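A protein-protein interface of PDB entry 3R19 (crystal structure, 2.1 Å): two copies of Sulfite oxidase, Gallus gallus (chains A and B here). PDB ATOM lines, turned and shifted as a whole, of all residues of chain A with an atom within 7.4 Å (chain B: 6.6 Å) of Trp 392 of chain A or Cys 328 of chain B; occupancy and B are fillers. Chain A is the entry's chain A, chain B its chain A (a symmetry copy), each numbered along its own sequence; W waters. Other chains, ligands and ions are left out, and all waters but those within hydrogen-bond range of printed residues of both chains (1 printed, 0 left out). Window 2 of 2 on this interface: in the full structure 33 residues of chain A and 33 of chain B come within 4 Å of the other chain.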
ATOM      1  N   ARG A 381     -16.027  20.879  -6.520  1.00  0.00           N
ATOM      2  CA  ARG A 381     -15.190  21.021  -5.327  1.00  0.00           C
ATOM      3  C   ARG A 381     -15.861  21.952  -4.326  1.00  0.00           C
ATOM      4  O   ARG A 381     -16.574  22.878  -4.712  1.00  0.00           O
ATOM      5  CB  ARG A 381     -13.786  21.557  -5.688  1.00  0.00           C
ATOM      6  CG  ARG A 381     -12.722  21.283  -4.616  1.00  0.00           C
ATOM      7  CD  ARG A 381     -11.325  21.791  -5.012  1.00  0.00           C
ATOM      8  NE  ARG A 381     -11.231  23.250  -4.865  1.00  0.00           N
ATOM      9  CZ  ARG A 381     -11.171  24.114  -5.879  1.00  0.00           C
ATOM     10  NH1 ARG A 381     -11.179  23.689  -7.134  1.00  0.00           N
ATOM     11  NH2 ARG A 381     -11.082  25.414  -5.638  1.00  0.00           N
ATOM     12  N   VAL A 382     -15.641  21.684  -3.041  1.00  0.00           N
ATOM     13  CA  VAL A 382     -16.003  22.607  -1.973  1.00  0.00           C
ATOM     14  C   VAL A 382     -14.770  22.799  -1.103  1.00  0.00           C
ATOM     15  O   VAL A 382     -14.179  21.819  -0.617  1.00  0.00           O
ATOM     16  CB  VAL A 382     -17.208  22.098  -1.128  1.00  0.00           C
ATOM     17  CG1 VAL A 382     -17.403  22.944   0.138  1.00  0.00           C
ATOM     18  CG2 VAL A 382     -18.498  22.090  -1.959  1.00  0.00           C
ATOM     19  N   ASP A 383     -14.365  24.060  -0.952  1.00  0.00           N
ATOM     20  CA  ASP A 383     -13.239  24.448  -0.103  1.00  0.00           C
ATOM     21  C   ASP A 383     -13.776  24.891   1.235  1.00  0.00           C
ATOM     22  O   ASP A 383     -14.782  25.596   1.286  1.00  0.00           O
ATOM     23  CB  ASP A 383     -12.463  25.604  -0.739  1.00  0.00           C
ATOM     24  CG  ASP A 383     -11.746  25.202  -2.016  1.00  0.00           C
ATOM     25  OD1 ASP A 383     -11.261  24.046  -2.101  1.00  0.00           O
ATOM     26  OD2 ASP A 383     -11.669  26.049  -2.937  1.00  0.00           O
ATOM     27  N   VAL A 384     -13.114  24.476   2.316  1.00  0.00           N
ATOM     28  CA  VAL A 384     -13.532  24.831   3.675  1.00  0.00           C
ATOM     29  C   VAL A 384     -12.351  25.412   4.471  1.00  0.00           C
ATOM     30  O   VAL A 384     -11.250  24.858   4.467  1.00  0.00           O
ATOM     31  CB  VAL A 384     -14.150  23.618   4.444  1.00  0.00           C
ATOM     32  CG1 VAL A 384     -14.529  24.010   5.872  1.00  0.00           C
ATOM     33  CG2 VAL A 384     -15.374  23.079   3.712  1.00  0.00           C
ATOM     34  N   SER A 385     -12.611  26.534   5.139  1.00  0.00           N
ATOM     35  CA  SER A 385     -11.620  27.245   5.933  1.00  0.00           C
ATOM     36  C   SER A 385     -12.100  27.341   7.372  1.00  0.00           C
ATOM     37  O   SER A 385     -13.304  27.359   7.620  1.00  0.00           O
ATOM     38  CB  SER A 385     -11.428  28.657   5.368  1.00  0.00           C
ATOM     39  OG  SER A 385     -10.506  29.401   6.153  1.00  0.00           O
ATOM     40  N   LEU A 386     -11.155  27.411   8.310  1.00  0.00           N
ATOM     41  CA  LEU A 386     -11.464  27.588   9.735  1.00  0.00           C
ATOM     42  C   LEU A 386     -10.904  28.906  10.261  1.00  0.00           C
ATOM     43  O   LEU A 386     -11.092  29.250  11.436  1.00  0.00           O
ATOM     44  CB  LEU A 386     -10.858  26.451  10.566  1.00  0.00           C
ATOM     45  CG  LEU A 386     -10.947  25.004  10.082  1.00  0.00           C
ATOM     46  CD1 LEU A 386     -10.154  24.105  11.033  1.00  0.00           C
ATOM     47  CD2 LEU A 386     -12.395  24.533   9.947  1.00  0.00           C
ATOM     48  N   ASP A 387     -10.200  29.633   9.397  1.00  0.00           N
ATOM     49  CA  ASP A 387      -9.488  30.834   9.826  1.00  0.00           C
ATOM     50  C   ASP A 387      -9.936  32.067   9.035  1.00  0.00           C
ATOM     51  O   ASP A 387      -9.138  32.965   8.762  1.00  0.00           O
ATOM     52  CB  ASP A 387      -7.964  30.613   9.763  1.00  0.00           C
ATOM     53  CG  ASP A 387      -7.460  30.289   8.352  1.00  0.00           C
ATOM     54  OD1 ASP A 387      -8.259  30.292   7.390  1.00  0.00           O
ATOM     55  OD2 ASP A 387      -6.248  30.036   8.203  1.00  0.00           O
ATOM     56  N   GLY A 388     -11.219  32.094   8.671  1.00  0.00           N
ATOM     57  CA  GLY A 388     -11.820  33.248   8.011  1.00  0.00           C
ATOM     58  C   GLY A 388     -11.522  33.349   6.527  1.00  0.00           C
ATOM     59  O   GLY A 388     -11.708  34.404   5.923  1.00  0.00           O
ATOM     60  N   GLY A 389     -11.050  32.257   5.937  1.00  0.00           N
ATOM     61  CA  GLY A 389     -10.791  32.224   4.504  1.00  0.00           C
ATOM     62  C   GLY A 389      -9.360  32.520   4.102  1.00  0.00           C
ATOM     63  O   GLY A 389      -9.096  32.874   2.950  1.00  0.00           O
ATOM     64  N   ARG A 390      -8.441  32.380   5.054  1.00  0.00           N
ATOM     65  CA  ARG A 390      -7.016  32.551   4.791  1.00  0.00           C
ATOM     66  C   ARG A 390      -6.414  31.263   4.231  1.00  0.00           C
ATOM     67  O   ARG A 390      -5.714  31.290   3.214  1.00  0.00           O
ATOM     68  CB  ARG A 390      -6.279  33.000   6.054  1.00  0.00           C
ATOM     69  CG  ARG A 390      -6.593  34.439   6.472  1.00  0.00           C
ATOM     70  CD  ARG A 390      -6.165  34.708   7.921  1.00  0.00           C
ATOM     71  NE  ARG A 390      -6.129  36.138   8.235  1.00  0.00           N
ATOM     72  CZ  ARG A 390      -5.020  36.823   8.514  1.00  0.00           C
ATOM     73  NH1 ARG A 390      -3.839  36.216   8.534  1.00  0.00           N
ATOM     74  NH2 ARG A 390      -5.089  38.121   8.790  1.00  0.00           N
ATOM     75  N   THR A 391      -6.702  30.141   4.891  1.00  0.00           N
ATOM     76  CA  THR A 391      -6.265  28.823   4.422  1.00  0.00           C
ATOM     77  C   THR A 391      -7.479  27.919   4.203  1.00  0.00           C
ATOM     78  O   THR A 391      -8.507  28.082   4.863  1.00  0.00           O
ATOM     79  CB  THR A 391      -5.303  28.136   5.417  1.00  0.00           C
ATOM     80  OG1 THR A 391      -5.972  27.947   6.667  1.00  0.00           O
ATOM     81  CG2 THR A 391      -4.033  28.970   5.638  1.00  0.00           C
ATOM     82  N   TRP A 392      -7.346  26.962   3.290  1.00  0.00           N
ATOM     83  CA  TRP A 392      -8.472  26.130   2.871  1.00  0.00           C
ATOM     84  C   TRP A 392      -8.112  24.656   2.844  1.00  0.00           C
ATOM     85  O   TRP A 392      -6.950  24.308   2.657  1.00  0.00           O
ATOM     86  CB  TRP A 392      -8.931  26.544   1.471  1.00  0.00           C
ATOM     87  CG  TRP A 392      -9.303  27.983   1.373  1.00  0.00           C
ATOM     88  CD1 TRP A 392      -8.469  29.033   1.080  1.00  0.00           C
ATOM     89  CD2 TRP A 392     -10.606  28.542   1.568  1.00  0.00           C
ATOM     90  NE1 TRP A 392      -9.186  30.215   1.073  1.00  0.00           N
ATOM     91  CE2 TRP A 392     -10.496  29.942   1.371  1.00  0.00           C
ATOM     92  CE3 TRP A 392     -11.861  27.999   1.886  1.00  0.00           C
ATOM     93  CZ2 TRP A 392     -11.594  30.805   1.494  1.00  0.00           C
ATOM     94  CZ3 TRP A 392     -12.958  28.864   1.998  1.00  0.00           C
ATOM     95  CH2 TRP A 392     -12.809  30.248   1.808  1.00  0.00           C
ATOM     96  N   LYS A 393      -9.118  23.807   3.038  1.00  0.00           N
ATOM     97  CA  LYS A 393      -9.006  22.357   2.849  1.00  0.00           C
ATOM     98  C   LYS A 393     -10.157  21.906   1.951  1.00  0.00           C
ATOM     99  O   LYS A 393     -11.187  22.568   1.906  1.00  0.00           O
ATOM    100  CB  LYS A 393      -9.089  21.621   4.186  1.00  0.00           C
ATOM    101  CG  LYS A 393      -7.916  21.867   5.131  1.00  0.00           C
ATOM    102  CD  LYS A 393      -8.172  21.214   6.481  1.00  0.00           C
ATOM    103  CE  LYS A 393      -7.726  22.108   7.647  1.00  0.00           C
ATOM    104  NZ  LYS A 393      -6.387  22.703   7.398  1.00  0.00           N
ATOM    105  N   VAL A 394      -9.990  20.781   1.259  1.00  0.00           N
ATOM    106  CA  VAL A 394     -11.011  20.278   0.327  1.00  0.00           C
ATOM    107  C   VAL A 394     -11.976  19.331   1.049  1.00  0.00           C
ATOM    108  O   VAL A 394     -11.552  18.342   1.633  1.00  0.00           O
ATOM    109  CB  VAL A 394     -10.360  19.554  -0.881  1.00  0.00           C
ATOM    110  CG1 VAL A 394     -11.418  19.023  -1.839  1.00  0.00           C
ATOM    111  CG2 VAL A 394      -9.405  20.494  -1.614  1.00  0.00           C
ATOM    112  N   LEU A 415     -16.345  17.687   6.188  1.00  0.00           N
ATOM    113  CA  LEU A 415     -14.912  17.668   6.433  1.00  0.00           C
ATOM    114  C   LEU A 415     -14.648  17.580   7.937  1.00  0.00           C
ATOM    115  O   LEU A 415     -15.137  18.411   8.705  1.00  0.00           O
ATOM    116  CB  LEU A 415     -14.235  18.917   5.862  1.00  0.00           C
ATOM    117  CG  LEU A 415     -12.724  19.049   6.068  1.00  0.00           C
ATOM    118  CD1 LEU A 415     -11.936  18.062   5.203  1.00  0.00           C
ATOM    119  CD2 LEU A 415     -12.278  20.482   5.812  1.00  0.00           C
ATOM    120  N   ILE A 427     -15.554  29.536  10.382  1.00  0.00           N
ATOM    121  CA  ILE A 427     -15.698  28.478   9.397  1.00  0.00           C
ATOM    122  C   ILE A 427     -16.331  29.055   8.132  1.00  0.00           C
ATOM    123  O   ILE A 427     -17.384  29.689   8.192  1.00  0.00           O
ATOM    124  CB  ILE A 427     -16.537  27.302   9.949  1.00  0.00           C
ATOM    125  CG1 ILE A 427     -15.943  26.798  11.277  1.00  0.00           C
ATOM    126  CG2 ILE A 427     -16.637  26.177   8.918  1.00  0.00           C
ATOM    127  CD1 ILE A 427     -16.815  25.804  12.014  1.00  0.00           C
ATOM    128  N   VAL A 428     -15.664  28.845   6.999  1.00  0.00           N
ATOM    129  CA  VAL A 428     -16.098  29.384   5.707  1.00  0.00           C
ATOM    130  C   VAL A 428     -16.142  28.260   4.680  1.00  0.00           C
ATOM    131  O   VAL A 428     -15.273  27.392   4.673  1.00  0.00           O
ATOM    132  CB  VAL A 428     -15.137  30.478   5.185  1.00  0.00           C
ATOM    133  CG1 VAL A 428     -15.721  31.182   3.956  1.00  0.00           C
ATOM    134  CG2 VAL A 428     -14.790  31.496   6.279  1.00  0.00           C
ATOM    135  N   CYS A 429     -17.159  28.265   3.822  1.00  0.00           N
ATOM    136  CA  CYS A 429     -17.188  27.342   2.694  1.00  0.00           C
ATOM    137  C   CYS A 429     -17.420  28.083   1.383  1.00  0.00           C
ATOM    138  O   CYS A 429     -18.113  29.107   1.343  1.00  0.00           O
ATOM    139  CB  CYS A 429     -18.238  26.242   2.906  1.00  0.00           C
ATOM    140  SG  CYS A 429     -19.968  26.794   2.752  1.00  0.00           S
ATOM    141  N   LYS A 430     -16.819  27.577   0.312  1.00  0.00           N
ATOM    142  CA  LYS A 430     -17.067  28.103  -1.029  1.00  0.00           C
ATOM    143  C   LYS A 430     -17.027  26.961  -2.021  1.00  0.00           C
ATOM    144  O   LYS A 430     -16.212  26.043  -1.881  1.00  0.00           O
ATOM    145  CB  LYS A 430     -16.065  29.204  -1.410  1.00  0.00           C
ATOM    146  CG  LYS A 430     -14.600  28.779  -1.521  1.00  0.00           C
ATOM    147  CD  LYS A 430     -13.701  30.007  -1.660  1.00  0.00           C
ATOM    148  CE  LYS A 430     -12.223  29.637  -1.683  1.00  0.00           C
ATOM    149  NZ  LYS A 430     -11.816  28.883  -2.907  1.00  0.00           N
ATOM    150  N   ALA A 431     -17.905  27.024  -3.023  1.00  0.00           N
ATOM    151  CA  ALA A 431     -18.046  25.935  -3.982  1.00  0.00           C
ATOM    152  C   ALA A 431     -17.648  26.361  -5.380  1.00  0.00           C
ATOM    153  O   ALA A 431     -17.688  27.552  -5.715  1.00  0.00           O
ATOM    154  CB  ALA A 431     -19.485  25.383  -3.973  1.00  0.00           C
ATOM    155  N   ASP A 441     -16.044  36.690  -2.432  1.00  0.00           N
ATOM    156  CA  ASP A 441     -15.617  36.816  -1.030  1.00  0.00           C
ATOM    157  C   ASP A 441     -16.663  37.429  -0.109  1.00  0.00           C
ATOM    158  O   ASP A 441     -16.843  36.965   1.025  1.00  0.00           O
ATOM    159  CB  ASP A 441     -14.353  37.679  -0.886  1.00  0.00           C
ATOM    160  CG  ASP A 441     -13.212  37.237  -1.774  1.00  0.00           C
ATOM    161  OD1 ASP A 441     -13.444  36.712  -2.886  1.00  0.00           O
ATOM    162  OD2 ASP A 441     -12.052  37.469  -1.371  1.00  0.00           O
ATOM    163  N   TRP A 457     -19.416  33.974   0.333  1.00  0.00           N
ATOM    164  CA  TRP A 457     -19.064  32.868   1.229  1.00  0.00           C
ATOM    165  C   TRP A 457     -19.869  32.926   2.520  1.00  0.00           C
ATOM    166  O   TRP A 457     -19.948  33.974   3.175  1.00  0.00           O
ATOM    167  CB  TRP A 457     -17.580  32.861   1.599  1.00  0.00           C
ATOM    168  CG  TRP A 457     -16.596  32.999   0.470  1.00  0.00           C
ATOM    169  CD1 TRP A 457     -16.776  32.658  -0.846  1.00  0.00           C
ATOM    170  CD2 TRP A 457     -15.252  33.475   0.580  1.00  0.00           C
ATOM    171  NE1 TRP A 457     -15.629  32.915  -1.560  1.00  0.00           N
ATOM    172  CE2 TRP A 457     -14.678  33.415  -0.708  1.00  0.00           C
ATOM    173  CE3 TRP A 457     -14.477  33.958   1.646  1.00  0.00           C
ATOM    174  CZ2 TRP A 457     -13.369  33.823  -0.961  1.00  0.00           C
ATOM    175  CZ3 TRP A 457     -13.173  34.362   1.394  1.00  0.00           C
ATOM    176  CH2 TRP A 457     -12.633  34.287   0.103  1.00  0.00           C
ATOM    177  N   HIS A 458     -20.448  31.788   2.884  1.00  0.00           N
ATOM    178  CA  HIS A 458     -21.089  31.635   4.177  1.00  0.00           C
ATOM    179  C   HIS A 458     -20.021  31.488   5.264  1.00  0.00           C
ATOM    180  O   HIS A 458     -19.089  30.687   5.117  1.00  0.00           O
ATOM    181  CB  HIS A 458     -22.038  30.440   4.157  1.00  0.00           C
ATOM    182  CG  HIS A 458     -22.892  30.329   5.382  1.00  0.00           C
ATOM    183  ND1 HIS A 458     -23.113  29.133   6.026  1.00  0.00           N
ATOM    184  CD2 HIS A 458     -23.565  31.267   6.088  1.00  0.00           C
ATOM    185  CE1 HIS A 458     -23.904  29.333   7.064  1.00  0.00           C
ATOM    186  NE2 HIS A 458     -24.184  30.622   7.130  1.00  0.00           N
ATOM    187  N   ARG A 459     -20.161  32.286   6.329  1.00  0.00           N
ATOM    188  CA  ARG A 459     -19.212  32.339   7.444  1.00  0.00           C
ATOM    189  C   ARG A 459     -19.905  32.027   8.769  1.00  0.00           C
ATOM    190  O   ARG A 459     -20.922  32.637   9.113  1.00  0.00           O
ATOM    191  CB  ARG A 459     -18.540  33.718   7.537  1.00  0.00           C
ATOM    192  CG  ARG A 459     -17.722  34.112   6.298  1.00  0.00           C
ATOM    193  CD  ARG A 459     -17.389  35.606   6.316  1.00  0.00           C
ATOM    194  NE  ARG A 459     -16.805  36.053   5.051  1.00  0.00           N
ATOM    195  CZ  ARG A 459     -15.499  36.120   4.791  1.00  0.00           C
ATOM    196  NH1 ARG A 459     -14.605  35.772   5.708  1.00  0.00           N
ATOM    197  NH2 ARG A 459     -15.087  36.548   3.606  1.00  0.00           N
ATOM    198  N   ARG B 197       1.707  34.259  -5.026  1.00  0.00           N
ATOM    199  CA  ARG B 197       2.698  33.208  -4.843  1.00  0.00           C
ATOM    200  C   ARG B 197       3.078  32.772  -6.250  1.00  0.00           C
ATOM    201  O   ARG B 197       2.193  32.641  -7.102  1.00  0.00           O
ATOM    202  CB  ARG B 197       2.066  32.038  -4.083  1.00  0.00           C
ATOM    203  CG  ARG B 197       3.015  30.919  -3.676  1.00  0.00           C
ATOM    204  CD  ARG B 197       2.309  29.879  -2.803  1.00  0.00           C
ATOM    205  NE  ARG B 197       1.588  30.491  -1.681  1.00  0.00           N
ATOM    206  CZ  ARG B 197       0.267  30.421  -1.489  1.00  0.00           C
ATOM    207  NH1 ARG B 197      -0.504  29.746  -2.332  1.00  0.00           N
ATOM    208  NH2 ARG B 197      -0.287  31.021  -0.439  1.00  0.00           N
ATOM    209  N   PHE B 325      -7.440  23.611  -9.476  1.00  0.00           N
ATOM    210  CA  PHE B 325      -7.311  22.954  -8.174  1.00  0.00           C
ATOM    211  C   PHE B 325      -7.516  23.929  -7.037  1.00  0.00           C
ATOM    212  O   PHE B 325      -7.512  25.142  -7.248  1.00  0.00           O
ATOM    213  CB  PHE B 325      -5.935  22.272  -8.041  1.00  0.00           C
ATOM    214  CG  PHE B 325      -5.740  21.143  -9.004  1.00  0.00           C
ATOM    215  CD1 PHE B 325      -6.266  19.879  -8.727  1.00  0.00           C
ATOM    216  CD2 PHE B 325      -5.076  21.353 -10.216  1.00  0.00           C
ATOM    217  CE1 PHE B 325      -6.110  18.832  -9.630  1.00  0.00           C
ATOM    218  CE2 PHE B 325      -4.916  20.310 -11.130  1.00  0.00           C
ATOM    219  CZ  PHE B 325      -5.436  19.046 -10.836  1.00  0.00           C
ATOM    220  N   SER B 326      -7.686  23.381  -5.831  1.00  0.00           N
ATOM    221  CA  SER B 326      -7.830  24.158  -4.612  1.00  0.00           C
ATOM    222  C   SER B 326      -6.555  24.972  -4.319  1.00  0.00           C
ATOM    223  O   SER B 326      -5.455  24.566  -4.713  1.00  0.00           O
ATOM    224  CB  SER B 326      -8.146  23.222  -3.438  1.00  0.00           C
ATOM    225  OG  SER B 326      -8.360  23.949  -2.235  1.00  0.00           O
ATOM    226  N   PRO B 327      -6.695  26.121  -3.625  1.00  0.00           N
ATOM    227  CA  PRO B 327      -5.499  26.905  -3.288  1.00  0.00           C
ATOM    228  C   PRO B 327      -4.496  26.170  -2.380  1.00  0.00           C
ATOM    229  O   PRO B 327      -3.332  26.543  -2.355  1.00  0.00           O
ATOM    230  CB  PRO B 327      -6.059  28.161  -2.590  1.00  0.00           C
ATOM    231  CG  PRO B 327      -7.517  27.874  -2.336  1.00  0.00           C
ATOM    232  CD  PRO B 327      -7.946  26.831  -3.301  1.00  0.00           C
ATOM    233  N   CYS B 328      -4.939  25.131  -1.673  1.00  0.00           N
ATOM    234  CA  CYS B 328      -4.055  24.347  -0.793  1.00  0.00           C
ATOM    235  C   CYS B 328      -3.138  23.376  -1.552  1.00  0.00           C
ATOM    236  O   CYS B 328      -2.132  22.909  -1.009  1.00  0.00           O
ATOM    237  CB  CYS B 328      -4.871  23.575   0.260  1.00  0.00           C
ATOM    238  SG  CYS B 328      -5.981  22.275  -0.402  1.00  0.00           S
ATOM    239  N   VAL B 329      -3.482  23.080  -2.805  1.00  0.00           N
ATOM    240  CA  VAL B 329      -2.765  22.059  -3.574  1.00  0.00           C
ATOM    241  C   VAL B 329      -1.413  22.561  -4.114  1.00  0.00           C
ATOM    242  O   VAL B 329      -1.316  23.665  -4.663  1.00  0.00           O
ATOM    243  CB  VAL B 329      -3.662  21.459  -4.702  1.00  0.00           C
ATOM    244  CG1 VAL B 329      -2.858  20.574  -5.647  1.00  0.00           C
ATOM    245  CG2 VAL B 329      -4.814  20.663  -4.090  1.00  0.00           C
ATOM    246  N   ASP B 330      -0.383  21.735  -3.932  1.00  0.00           N
ATOM    247  CA  ASP B 330       0.972  22.025  -4.404  1.00  0.00           C
ATOM    248  C   ASP B 330       1.470  20.842  -5.249  1.00  0.00           C
ATOM    249  O   ASP B 330       0.757  19.843  -5.405  1.00  0.00           O
ATOM    250  CB  ASP B 330       1.908  22.299  -3.209  1.00  0.00           C
ATOM    251  CG  ASP B 330       3.121  23.166  -3.581  1.00  0.00           C
ATOM    252  OD1 ASP B 330       3.293  23.525  -4.771  1.00  0.00           O
ATOM    253  OD2 ASP B 330       3.915  23.490  -2.671  1.00  0.00           O
ATOM    254  N   ASP B 332       3.667  18.546  -4.763  1.00  0.00           N
ATOM    255  CA  ASP B 332       3.808  17.291  -4.026  1.00  0.00           C
ATOM    256  C   ASP B 332       2.487  16.533  -3.840  1.00  0.00           C
ATOM    257  O   ASP B 332       2.504  15.337  -3.561  1.00  0.00           O
ATOM    258  CB  ASP B 332       4.497  17.519  -2.670  1.00  0.00           C
ATOM    259  CG  ASP B 332       3.851  18.637  -1.849  1.00  0.00           C
ATOM    260  OD1 ASP B 332       2.925  19.328  -2.347  1.00  0.00           O
ATOM    261  OD2 ASP B 332       4.289  18.830  -0.692  1.00  0.00           O
ATOM    262  N   THR B 333       1.351  17.218  -4.002  1.00  0.00           N
ATOM    263  CA  THR B 333       0.048  16.608  -3.698  1.00  0.00           C
ATOM    264  C   THR B 333      -0.956  16.615  -4.852  1.00  0.00           C
ATOM    265  O   THR B 333      -2.029  16.019  -4.737  1.00  0.00           O
ATOM    266  CB  THR B 333      -0.632  17.262  -2.464  1.00  0.00           C
ATOM    267  OG1 THR B 333      -0.908  18.640  -2.736  1.00  0.00           O
ATOM    268  CG2 THR B 333       0.245  17.143  -1.205  1.00  0.00           C
ATOM    269  N   ALA B 444      -6.266  35.580  -4.052  1.00  0.00           N
ATOM    270  CA  ALA B 444      -5.731  34.567  -3.122  1.00  0.00           C
ATOM    271  C   ALA B 444      -6.605  33.304  -2.947  1.00  0.00           C
ATOM    272  O   ALA B 444      -6.100  32.197  -3.088  1.00  0.00           O
ATOM    273  CB  ALA B 444      -5.344  35.186  -1.754  1.00  0.00           C
ATOM    274  N   PRO B 445      -7.921  33.461  -2.680  1.00  0.00           N
ATOM    275  CA  PRO B 445      -8.806  32.291  -2.486  1.00  0.00           C
ATOM    276  C   PRO B 445      -9.067  31.445  -3.746  1.00  0.00           C
ATOM    277  O   PRO B 445      -9.553  30.322  -3.635  1.00  0.00           O
ATOM    278  CB  PRO B 445     -10.118  32.924  -2.013  1.00  0.00           C
ATOM    279  CG  PRO B 445      -9.718  34.298  -1.487  1.00  0.00           C
ATOM    280  CD  PRO B 445      -8.649  34.721  -2.434  1.00  0.00           C
ATOM    281  N   ILE B 446      -8.754  31.984  -4.918  1.00  0.00           N
ATOM    282  CA  ILE B 446      -8.811  31.213  -6.170  1.00  0.00           C
ATOM    283  C   ILE B 446      -7.418  30.841  -6.708  1.00  0.00           C
ATOM    284  O   ILE B 446      -7.289  30.320  -7.828  1.00  0.00           O
ATOM    285  CB  ILE B 446      -9.625  31.942  -7.257  1.00  0.00           C
ATOM    286  CG1 ILE B 446      -8.997  33.309  -7.582  1.00  0.00           C
ATOM    287  CG2 ILE B 446     -11.099  32.077  -6.825  1.00  0.00           C
ATOM    288  CD1 ILE B 446      -9.431  33.910  -8.921  1.00  0.00           C
ATOM    289  N   TRP B 447      -6.380  31.108  -5.916  1.00  0.00           N
ATOM    290  CA  TRP B 447      -5.012  30.772  -6.305  1.00  0.00           C
ATOM    291  C   TRP B 447      -4.913  29.269  -6.552  1.00  0.00           C
ATOM    292  O   TRP B 447      -5.636  28.485  -5.943  1.00  0.00           O
ATOM    293  CB  TRP B 447      -4.003  31.193  -5.226  1.00  0.00           C
ATOM    294  CG  TRP B 447      -2.554  30.995  -5.655  1.00  0.00           C
ATOM    295  CD1 TRP B 447      -1.753  31.907  -6.281  1.00  0.00           C
ATOM    296  CD2 TRP B 447      -1.763  29.806  -5.504  1.00  0.00           C
ATOM    297  NE1 TRP B 447      -0.514  31.360  -6.537  1.00  0.00           N
ATOM    298  CE2 TRP B 447      -0.492  30.074  -6.065  1.00  0.00           C
ATOM    299  CE3 TRP B 447      -2.004  28.541  -4.946  1.00  0.00           C
ATOM    300  CZ2 TRP B 447       0.543  29.125  -6.071  1.00  0.00           C
ATOM    301  CZ3 TRP B 447      -0.977  27.596  -4.963  1.00  0.00           C
ATOM    302  CH2 TRP B 447       0.279  27.895  -5.523  1.00  0.00           C
HETATM  303  O   HOH W   1      -7.403  19.325   1.462  1.00  0.00           O
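Hydrophobic or aromatic side chains of chain B within 4 Å of the printed part of chain A: Pro 327 and Pro 445.
Along chain A the printed residues that touch a printed residue of chain B span positions 381 to 457.
Among the printed residues, 10 pairs touch across the chains.
Val 384 of chain A touches none of the printed residues of chain B.
Of the printed residues of chain B, Trp 392 of chain A touches Pro 327 (3.7 Å) and Cys 328 (3.3 Å).
Printed residues of chain B within 4 Å of Lys 430 of chain A: Pro 445.
Of the printed residues of chain B, Trp 457 of chain A touches Pro 445 (3.3 Å).
Printed residues of chain A within 4 Å of Pro 327 of chain B: Asp 383 and Trp 392.
The nearest residue of chain A that does not touch Cys 328 of chain B is Val 394 of chain A (4.05 Å).
Arg 381 of chain A touches Phe 325 of chain B.
Arg 381 of chain A touches Ser 326 of chain B (NE to CB, 3.4 Å).
CD of Pro 327 of chain B touches OD2 of Asp 383 of chain A (3.8 Å).
Trp 392 of chain A touches Pro 327 of chain B.
CB of Ser 326 of chain B touches CG2 of Val 394 of chain A, at 3.5 Å.
OD2 of Asp 441 of chain A touches CG of Pro 445 of chain B, 3.9 Å away.
Trp 457 of chain A touches Pro 445 of chain B (CH2 to CG, 3.3 Å).
The side-chain carboxylate of Asp 383 of chain A lies within salt-bridge range of the guanidinium group of Arg 381 of chain A.
The side-chain amino group of Lys 430 of chain A lies within salt-bridge range of the side-chain carboxylate of Asp 383 of chain A (2.8 Å).
O of Gly 389 of chain A is in hydrogen-bond range of NE1 of Trp 392 of chain A (3.3 Å).
The backbone carbonyl oxygen (O) of Asp 441 of chain A lies within hydrogen-bond range of the guanidinium group (NH2) of Arg 459 of chain A, 3.1 Å away.
The side-chain hydroxyl (OG) of Ser 326 of chain B lies within hydrogen-bond range of the side-chain sulfur (SG) of Cys 328 of chain B (3.4 Å).
Water W1 lies within hydrogen-bond range of N of Val 394 of chain A (3.0 Å) and SG of Cys 328 of chain B (3.8 Å).
No position is printed for both chains.
The side-chain hydroxyl (OG) of Ser 326 of chain B sits at hydrogen-bond distance from the side-chain carboxylate (OD1) of Asp 383 of chain A, 2.9 Å away.
O of Trp 392 of chain A sits close to SG of Cys 328 of chain B, 3.8 Å away.
NZ of Lys 430 of chain A is in hydrogen-bond range of O of Pro 445 of chain B, 2.8 Å away.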
